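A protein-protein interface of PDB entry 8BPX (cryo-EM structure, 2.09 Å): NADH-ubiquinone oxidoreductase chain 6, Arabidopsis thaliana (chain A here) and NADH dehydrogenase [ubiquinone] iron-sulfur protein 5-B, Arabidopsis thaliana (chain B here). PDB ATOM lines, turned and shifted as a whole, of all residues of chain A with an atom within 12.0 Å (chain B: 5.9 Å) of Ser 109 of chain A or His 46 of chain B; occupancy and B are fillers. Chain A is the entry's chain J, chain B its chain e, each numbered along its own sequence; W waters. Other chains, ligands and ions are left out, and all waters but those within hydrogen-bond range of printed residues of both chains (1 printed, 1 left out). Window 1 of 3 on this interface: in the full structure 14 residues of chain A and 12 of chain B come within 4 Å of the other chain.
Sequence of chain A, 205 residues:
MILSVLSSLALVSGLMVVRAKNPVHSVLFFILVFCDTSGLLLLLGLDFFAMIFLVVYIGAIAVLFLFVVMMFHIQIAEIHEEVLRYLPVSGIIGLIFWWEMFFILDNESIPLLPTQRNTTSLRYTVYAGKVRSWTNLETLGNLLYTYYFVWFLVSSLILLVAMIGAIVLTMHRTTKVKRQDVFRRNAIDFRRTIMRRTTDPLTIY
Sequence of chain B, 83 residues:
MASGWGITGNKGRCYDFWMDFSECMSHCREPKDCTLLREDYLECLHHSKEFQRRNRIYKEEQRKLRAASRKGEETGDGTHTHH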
ATOM      1  N   GLU A 100      14.058  -3.792 -20.053  1.00  0.00           N
ATOM      2  CA  GLU A 100      14.920  -4.339 -21.085  1.00  0.00           C
ATOM      3  C   GLU A 100      15.572  -5.645 -20.678  1.00  0.00           C
ATOM      4  O   GLU A 100      15.701  -6.556 -21.499  1.00  0.00           O
ATOM      5  CB  GLU A 100      16.031  -3.344 -21.400  1.00  0.00           C
ATOM      6  CG  GLU A 100      16.851  -3.766 -22.558  1.00  0.00           C
ATOM      7  CD  GLU A 100      16.167  -3.434 -23.839  1.00  0.00           C
ATOM      8  OE1 GLU A 100      15.680  -2.295 -23.959  1.00  0.00           O
ATOM      9  OE2 GLU A 100      16.082  -4.327 -24.707  1.00  0.00           O
ATOM     10  N   MET A 101      15.967  -5.750 -19.436  1.00  0.00           N
ATOM     11  CA  MET A 101      17.055  -6.622 -19.054  1.00  0.00           C
ATOM     12  C   MET A 101      16.601  -7.818 -18.223  1.00  0.00           C
ATOM     13  O   MET A 101      17.310  -8.824 -18.171  1.00  0.00           O
ATOM     14  CB  MET A 101      18.109  -5.769 -18.328  1.00  0.00           C
ATOM     15  CG  MET A 101      18.997  -6.445 -17.406  1.00  0.00           C
ATOM     16  SD  MET A 101      20.605  -6.603 -18.210  1.00  0.00           S
ATOM     17  CE  MET A 101      21.208  -4.910 -18.287  1.00  0.00           C
ATOM     18  N   PHE A 102      15.435  -7.738 -17.578  1.00  0.00           N
ATOM     19  CA  PHE A 102      14.792  -8.922 -17.006  1.00  0.00           C
ATOM     20  C   PHE A 102      14.097  -9.774 -18.058  1.00  0.00           C
ATOM     21  O   PHE A 102      13.805 -10.941 -17.792  1.00  0.00           O
ATOM     22  CB  PHE A 102      13.764  -8.525 -15.943  1.00  0.00           C
ATOM     23  CG  PHE A 102      14.363  -8.030 -14.667  1.00  0.00           C
ATOM     24  CD1 PHE A 102      15.004  -6.803 -14.621  1.00  0.00           C
ATOM     25  CD2 PHE A 102      14.265  -8.772 -13.505  1.00  0.00           C
ATOM     26  CE1 PHE A 102      15.552  -6.345 -13.443  1.00  0.00           C
ATOM     27  CE2 PHE A 102      14.807  -8.313 -12.326  1.00  0.00           C
ATOM     28  CZ  PHE A 102      15.450  -7.101 -12.296  1.00  0.00           C
ATOM     29  N   PHE A 103      13.829  -9.215 -19.241  1.00  0.00           N
ATOM     30  CA  PHE A 103      13.059  -9.890 -20.281  1.00  0.00           C
ATOM     31  C   PHE A 103      13.869 -10.126 -21.546  1.00  0.00           C
ATOM     32  O   PHE A 103      13.289 -10.442 -22.590  1.00  0.00           O
ATOM     33  CB  PHE A 103      11.798  -9.082 -20.609  1.00  0.00           C
ATOM     34  CG  PHE A 103      10.995  -8.700 -19.397  1.00  0.00           C
ATOM     35  CD1 PHE A 103      10.261  -9.652 -18.709  1.00  0.00           C
ATOM     36  CD2 PHE A 103      10.994  -7.395 -18.934  1.00  0.00           C
ATOM     37  CE1 PHE A 103       9.528  -9.306 -17.587  1.00  0.00           C
ATOM     38  CE2 PHE A 103      10.265  -7.045 -17.813  1.00  0.00           C
ATOM     39  CZ  PHE A 103       9.533  -8.003 -17.137  1.00  0.00           C
ATOM     40  N   ILE A 104      15.194  -9.979 -21.479  1.00  0.00           N
ATOM     41  CA  ILE A 104      16.037 -10.105 -22.663  1.00  0.00           C
ATOM     42  C   ILE A 104      16.021 -11.531 -23.202  1.00  0.00           C
ATOM     43  O   ILE A 104      16.098 -11.742 -24.417  1.00  0.00           O
ATOM     44  CB  ILE A 104      17.464  -9.624 -22.328  1.00  0.00           C
ATOM     45  CG1 ILE A 104      18.431  -9.857 -23.484  1.00  0.00           C
ATOM     46  CG2 ILE A 104      17.968 -10.295 -21.091  1.00  0.00           C
ATOM     47  CD1 ILE A 104      19.538  -8.840 -23.548  1.00  0.00           C
ATOM     48  N   LEU A 105      15.910 -12.524 -22.320  1.00  0.00           N
ATOM     49  CA  LEU A 105      15.891 -13.920 -22.736  1.00  0.00           C
ATOM     50  C   LEU A 105      14.538 -14.369 -23.275  1.00  0.00           C
ATOM     51  O   LEU A 105      14.459 -15.451 -23.866  1.00  0.00           O
ATOM     52  CB  LEU A 105      16.285 -14.829 -21.566  1.00  0.00           C
ATOM     53  CG  LEU A 105      17.635 -14.634 -20.872  1.00  0.00           C
ATOM     54  CD1 LEU A 105      18.008 -15.876 -20.075  1.00  0.00           C
ATOM     55  CD2 LEU A 105      18.726 -14.302 -21.867  1.00  0.00           C
ATOM     56  N   ASP A 106      13.480 -13.575 -23.092  1.00  0.00           N
ATOM     57  CA  ASP A 106      12.130 -14.054 -23.383  1.00  0.00           C
ATOM     58  C   ASP A 106      11.940 -14.373 -24.863  1.00  0.00           C
ATOM     59  O   ASP A 106      11.294 -15.368 -25.206  1.00  0.00           O
ATOM     60  CB  ASP A 106      11.100 -13.030 -22.911  1.00  0.00           C
ATOM     61  CG  ASP A 106      11.050 -12.918 -21.398  1.00  0.00           C
ATOM     62  OD1 ASP A 106      12.113 -13.055 -20.758  1.00  0.00           O
ATOM     63  OD2 ASP A 106       9.952 -12.701 -20.849  1.00  0.00           O
ATOM     64  N   ASN A 107      12.486 -13.546 -25.754  1.00  0.00           N
ATOM     65  CA  ASN A 107      12.305 -13.792 -27.181  1.00  0.00           C
ATOM     66  C   ASN A 107      13.190 -14.932 -27.671  1.00  0.00           C
ATOM     67  O   ASN A 107      12.792 -15.691 -28.561  1.00  0.00           O
ATOM     68  CB  ASN A 107      12.587 -12.520 -27.974  1.00  0.00           C
ATOM     69  CG  ASN A 107      11.390 -11.602 -28.038  1.00  0.00           C
ATOM     70  OD1 ASN A 107      10.529 -11.626 -27.158  1.00  0.00           O
ATOM     71  ND2 ASN A 107      11.328 -10.781 -29.079  1.00  0.00           N
ATOM     72  N   GLU A 108      14.388 -15.064 -27.106  1.00  0.00           N
ATOM     73  CA  GLU A 108      15.283 -16.140 -27.508  1.00  0.00           C
ATOM     74  C   GLU A 108      14.951 -17.438 -26.785  1.00  0.00           C
ATOM     75  O   GLU A 108      14.927 -18.507 -27.403  1.00  0.00           O
ATOM     76  CB  GLU A 108      16.733 -15.743 -27.245  1.00  0.00           C
ATOM     77  CG  GLU A 108      17.748 -16.595 -27.980  1.00  0.00           C
ATOM     78  CD  GLU A 108      17.799 -16.278 -29.461  1.00  0.00           C
ATOM     79  OE1 GLU A 108      16.973 -16.830 -30.218  1.00  0.00           O
ATOM     80  OE2 GLU A 108      18.664 -15.476 -29.869  1.00  0.00           O
ATOM     81  N   SER A 109      14.693 -17.362 -25.483  1.00  0.00           N
ATOM     82  CA  SER A 109      14.410 -18.531 -24.655  1.00  0.00           C
ATOM     83  C   SER A 109      12.971 -18.412 -24.165  1.00  0.00           C
ATOM     84  O   SER A 109      12.707 -17.897 -23.076  1.00  0.00           O
ATOM     85  CB  SER A 109      15.396 -18.626 -23.507  1.00  0.00           C
ATOM     86  OG  SER A 109      16.694 -18.927 -23.988  1.00  0.00           O
ATOM     87  N   ILE A 110      12.042 -18.891 -24.979  1.00  0.00           N
ATOM     88  CA  ILE A 110      10.619 -18.823 -24.644  1.00  0.00           C
ATOM     89  C   ILE A 110      10.305 -19.906 -23.616  1.00  0.00           C
ATOM     90  O   ILE A 110      10.630 -21.079 -23.847  1.00  0.00           O
ATOM     91  CB  ILE A 110       9.768 -18.989 -25.898  1.00  0.00           C
ATOM     92  CG1 ILE A 110       9.883 -17.744 -26.777  1.00  0.00           C
ATOM     93  CG2 ILE A 110       8.315 -19.247 -25.530  1.00  0.00           C
ATOM     94  CD1 ILE A 110       9.606 -17.997 -28.220  1.00  0.00           C
ATOM     95  N   PRO A 111       9.690 -19.563 -22.491  1.00  0.00           N
ATOM     96  CA  PRO A 111       9.413 -20.574 -21.467  1.00  0.00           C
ATOM     97  C   PRO A 111       8.380 -21.591 -21.925  1.00  0.00           C
ATOM     98  O   PRO A 111       7.486 -21.300 -22.721  1.00  0.00           O
ATOM     99  CB  PRO A 111       8.891 -19.750 -20.287  1.00  0.00           C
ATOM    100  CG  PRO A 111       8.356 -18.516 -20.898  1.00  0.00           C
ATOM    101  CD  PRO A 111       9.215 -18.228 -22.097  1.00  0.00           C
ATOM    102  N   LEU A 112       8.522 -22.804 -21.403  1.00  0.00           N
ATOM    103  CA  LEU A 112       7.526 -23.847 -21.600  1.00  0.00           C
ATOM    104  C   LEU A 112       6.438 -23.695 -20.543  1.00  0.00           C
ATOM    105  O   LEU A 112       6.702 -23.858 -19.348  1.00  0.00           O
ATOM    106  CB  LEU A 112       8.181 -25.223 -21.515  1.00  0.00           C
ATOM    107  CG  LEU A 112       7.324 -26.439 -21.857  1.00  0.00           C
ATOM    108  CD1 LEU A 112       6.974 -26.463 -23.340  1.00  0.00           C
ATOM    109  CD2 LEU A 112       8.033 -27.716 -21.442  1.00  0.00           C
ATOM    110  N   LEU A 113       5.224 -23.378 -20.977  1.00  0.00           N
ATOM    111  CA  LEU A 113       4.120 -23.234 -20.036  1.00  0.00           C
ATOM    112  C   LEU A 113       3.760 -24.595 -19.450  1.00  0.00           C
ATOM    113  O   LEU A 113       3.534 -25.549 -20.204  1.00  0.00           O
ATOM    114  CB  LEU A 113       2.906 -22.604 -20.718  1.00  0.00           C
ATOM    115  CG  LEU A 113       3.193 -21.292 -21.449  1.00  0.00           C
ATOM    116  CD1 LEU A 113       1.948 -20.745 -22.117  1.00  0.00           C
ATOM    117  CD2 LEU A 113       3.779 -20.271 -20.485  1.00  0.00           C
ATOM    118  N   ARG B  13      25.635 -31.218 -25.853  1.00  0.00           N
ATOM    119  CA  ARG B  13      24.355 -31.556 -26.473  1.00  0.00           C
ATOM    120  C   ARG B  13      24.252 -31.019 -27.896  1.00  0.00           C
ATOM    121  O   ARG B  13      23.757 -31.710 -28.793  1.00  0.00           O
ATOM    122  CB  ARG B  13      23.202 -31.025 -25.616  1.00  0.00           C
ATOM    123  CG  ARG B  13      21.900 -30.815 -26.388  1.00  0.00           C
ATOM    124  CD  ARG B  13      20.754 -30.356 -25.497  1.00  0.00           C
ATOM    125  NE  ARG B  13      20.534 -28.916 -25.566  1.00  0.00           N
ATOM    126  CZ  ARG B  13      20.819 -28.076 -24.580  1.00  0.00           C
ATOM    127  NH1 ARG B  13      21.325 -28.503 -23.435  1.00  0.00           N
ATOM    128  NH2 ARG B  13      20.586 -26.777 -24.746  1.00  0.00           N
ATOM    129  N   TYR B  41      21.222 -25.330 -34.958  1.00  0.00           N
ATOM    130  CA  TYR B  41      22.147 -25.061 -33.812  1.00  0.00           C
ATOM    131  C   TYR B  41      21.467 -24.157 -32.764  1.00  0.00           C
ATOM    132  O   TYR B  41      21.396 -24.575 -31.652  1.00  0.00           O
ATOM    133  CB  TYR B  41      23.487 -24.522 -34.327  1.00  0.00           C
ATOM    134  CG  TYR B  41      24.370 -24.022 -33.206  1.00  0.00           C
ATOM    135  CD1 TYR B  41      24.942 -24.906 -32.313  1.00  0.00           C
ATOM    136  CD2 TYR B  41      24.569 -22.667 -32.994  1.00  0.00           C
ATOM    137  CE1 TYR B  41      25.736 -24.468 -31.268  1.00  0.00           C
ATOM    138  CE2 TYR B  41      25.358 -22.203 -31.954  1.00  0.00           C
ATOM    139  CZ  TYR B  41      25.943 -23.112 -31.086  1.00  0.00           C
ATOM    140  OH  TYR B  41      26.723 -22.701 -30.056  1.00  0.00           O
ATOM    141  N   LEU B  42      20.899 -23.034 -33.189  1.00  0.00           N
ATOM    142  CA  LEU B  42      20.302 -22.121 -32.218  1.00  0.00           C
ATOM    143  C   LEU B  42      19.058 -22.721 -31.561  1.00  0.00           C
ATOM    144  O   LEU B  42      18.798 -22.462 -30.377  1.00  0.00           O
ATOM    145  CB  LEU B  42      19.985 -20.783 -32.881  1.00  0.00           C
ATOM    146  CG  LEU B  42      21.210 -20.010 -33.390  1.00  0.00           C
ATOM    147  CD1 LEU B  42      20.801 -18.698 -34.035  1.00  0.00           C
ATOM    148  CD2 LEU B  42      22.222 -19.764 -32.276  1.00  0.00           C
ATOM    149  N   GLU B  43      18.291 -23.529 -32.301  1.00  0.00           N
ATOM    150  CA  GLU B  43      17.166 -24.249 -31.713  1.00  0.00           C
ATOM    151  C   GLU B  43      17.637 -25.236 -30.655  1.00  0.00           C
ATOM    152  O   GLU B  43      17.000 -25.384 -29.608  1.00  0.00           O
ATOM    153  CB  GLU B  43      16.386 -24.976 -32.810  1.00  0.00           C
ATOM    154  CG  GLU B  43      15.189 -25.800 -32.334  1.00  0.00           C
ATOM    155  CD  GLU B  43      14.135 -24.983 -31.600  1.00  0.00           C
ATOM    156  OE1 GLU B  43      13.985 -23.780 -31.892  1.00  0.00           O
ATOM    157  OE2 GLU B  43      13.441 -25.552 -30.735  1.00  0.00           O
ATOM    158  N   CYS B  44      18.743 -25.934 -30.916  1.00  0.00           N
ATOM    159  CA  CYS B  44      19.308 -26.797 -29.886  1.00  0.00           C
ATOM    160  C   CYS B  44      19.717 -25.986 -28.663  1.00  0.00           C
ATOM    161  O   CYS B  44      19.547 -26.437 -27.524  1.00  0.00           O
ATOM    162  CB  CYS B  44      20.501 -27.578 -30.433  1.00  0.00           C
ATOM    163  SG  CYS B  44      21.247 -28.722 -29.247  1.00  0.00           S
ATOM    164  N   LEU B  45      20.193 -24.786 -28.772  1.00  0.00           N
ATOM    165  CA  LEU B  45      20.633 -23.997 -27.584  1.00  0.00           C
ATOM    166  C   LEU B  45      19.410 -23.550 -26.791  1.00  0.00           C
ATOM    167  O   LEU B  45      19.438 -23.683 -25.611  1.00  0.00           O
ATOM    168  CB  LEU B  45      21.359 -22.717 -27.969  1.00  0.00           C
ATOM    169  CG  LEU B  45      22.703 -22.834 -28.691  1.00  0.00           C
ATOM    170  CD1 LEU B  45      23.321 -21.458 -28.865  1.00  0.00           C
ATOM    171  CD2 LEU B  45      23.669 -23.752 -27.980  1.00  0.00           C
ATOM    172  N   HIS B  46      18.390 -23.065 -27.505  1.00  0.00           N
ATOM    173  CA  HIS B  46      17.329 -22.425 -26.732  1.00  0.00           C
ATOM    174  C   HIS B  46      15.958 -23.094 -26.803  1.00  0.00           C
ATOM    175  O   HIS B  46      15.079 -22.715 -26.022  1.00  0.00           O
ATOM    176  CB  HIS B  46      17.177 -20.954 -27.147  1.00  0.00           C
ATOM    177  CG  HIS B  46      18.479 -20.234 -27.312  1.00  0.00           C
ATOM    178  ND1 HIS B  46      19.290 -19.910 -26.247  1.00  0.00           N
ATOM    179  CD2 HIS B  46      19.104 -19.766 -28.418  1.00  0.00           C
ATOM    180  CE1 HIS B  46      20.363 -19.279 -26.689  1.00  0.00           C
ATOM    181  NE2 HIS B  46      20.275 -19.179 -28.003  1.00  0.00           N
ATOM    182  N   HIS B  47      15.743 -24.058 -27.700  1.00  0.00           N
ATOM    183  CA  HIS B  47      14.456 -24.755 -27.829  1.00  0.00           C
ATOM    184  C   HIS B  47      13.292 -23.791 -28.048  1.00  0.00           C
ATOM    185  O   HIS B  47      12.181 -24.035 -27.575  1.00  0.00           O
ATOM    186  CB  HIS B  47      14.162 -25.640 -26.613  1.00  0.00           C
ATOM    187  CG  HIS B  47      15.330 -26.449 -26.146  1.00  0.00           C
ATOM    188  ND1 HIS B  47      15.878 -27.467 -26.895  1.00  0.00           N
ATOM    189  CD2 HIS B  47      16.044 -26.403 -24.997  1.00  0.00           C
ATOM    190  CE1 HIS B  47      16.883 -28.007 -26.231  1.00  0.00           C
ATOM    191  NE2 HIS B  47      17.005 -27.379 -25.076  1.00  0.00           N
ATOM    192  N   SER B  48      13.527 -22.693 -28.765  1.00  0.00           N
ATOM    193  CA  SER B  48      12.508 -21.655 -28.873  1.00  0.00           C
ATOM    194  C   SER B  48      11.293 -22.142 -29.660  1.00  0.00           C
ATOM    195  O   SER B  48      10.151 -21.990 -29.211  1.00  0.00           O
ATOM    196  CB  SER B  48      13.105 -20.401 -29.511  1.00  0.00           C
ATOM    197  OG  SER B  48      12.111 -19.635 -30.164  1.00  0.00           O
ATOM    198  N   PHE B  51       9.289 -25.036 -27.789  1.00  0.00           N
ATOM    199  CA  PHE B  51       8.465 -24.541 -26.695  1.00  0.00           C
ATOM    200  C   PHE B  51       7.316 -23.686 -27.216  1.00  0.00           C
ATOM    201  O   PHE B  51       6.215 -23.721 -26.661  1.00  0.00           O
ATOM    202  CB  PHE B  51       9.329 -23.762 -25.700  1.00  0.00           C
ATOM    203  CG  PHE B  51      10.287 -24.628 -24.922  1.00  0.00           C
ATOM    204  CD1 PHE B  51      10.178 -26.007 -24.957  1.00  0.00           C
ATOM    205  CD2 PHE B  51      11.291 -24.063 -24.154  1.00  0.00           C
ATOM    206  CE1 PHE B  51      11.051 -26.805 -24.250  1.00  0.00           C
ATOM    207  CE2 PHE B  51      12.170 -24.858 -23.442  1.00  0.00           C
ATOM    208  CZ  PHE B  51      12.052 -26.228 -23.489  1.00  0.00           C
HETATM  209  O   HOH W   1      18.285 -20.892 -23.761  1.00  0.00           O
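OE1 of Glu 43 of chain B lies within hydrogen-bond range of N of Ser 48 of chain B (3.3 Å).
CB of His 46 of chain B touches O of Glu 108 of chain A, at 3.3 Å.
Ser 48 of chain B touches Glu 108 of chain A (CB to O, 3.4 Å).
ND1 of His 46 of chain B touches OG of Ser 109 of chain A, at 3.6 Å.
Ser 48 of chain B touches Ile 110 of chain A (OG to CD1, 3.6 Å).
Ile 110 of chain A touches Phe 51 of chain B (O to CD2, 3.1 Å).
CD1 of Leu 112 of chain A touches CD1 of Phe 51 of chain B, at 3.6 Å.
Ser 109 of chain A touches just one residue of chain B: His 46.
Of the printed residues of chain B, Ile 110 of chain A touches Ser 48 and Phe 51.
Of the printed residues of chain B, Leu 112 of chain A touches Phe 51 (3.6 Å).
No residue of chain A comes within 4 Å of Leu 42 of chain B.
No residue of chain A comes within 4 Å of Glu 43 of chain B.
Of chain A, only Glu 108 (3.3 Å) and Ser 109 (3.6 Å) come within 4 Å of His 46 of chain B.
Ser 48 of chain B touches just these residues of chain A: Glu 108 and Ile 110.
Of the printed residues of chain A, Phe 51 of chain B touches Ile 110 (3.1 Å) and Leu 112 (3.6 Å).
The nearest residue of chain A that does not touch His 46 of chain B is Ile 110 of chain A (5.0 Å).
The nearest printed residue of chain A that does not touch Phe 51 of chain B is Pro 111 of chain A (4.3 Å).
Of the 14 printed residues of chain A, 4 touch a printed residue of chain B.
Hydrophobic or aromatic side chains of chain A that line the printed part of chain B: Ile 110 and Leu 112.
Water W1 lies within hydrogen-bond range of OG of Ser 109 of chain A (2.5 Å) and ND1 of His 46 of chain B (2.9 Å).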
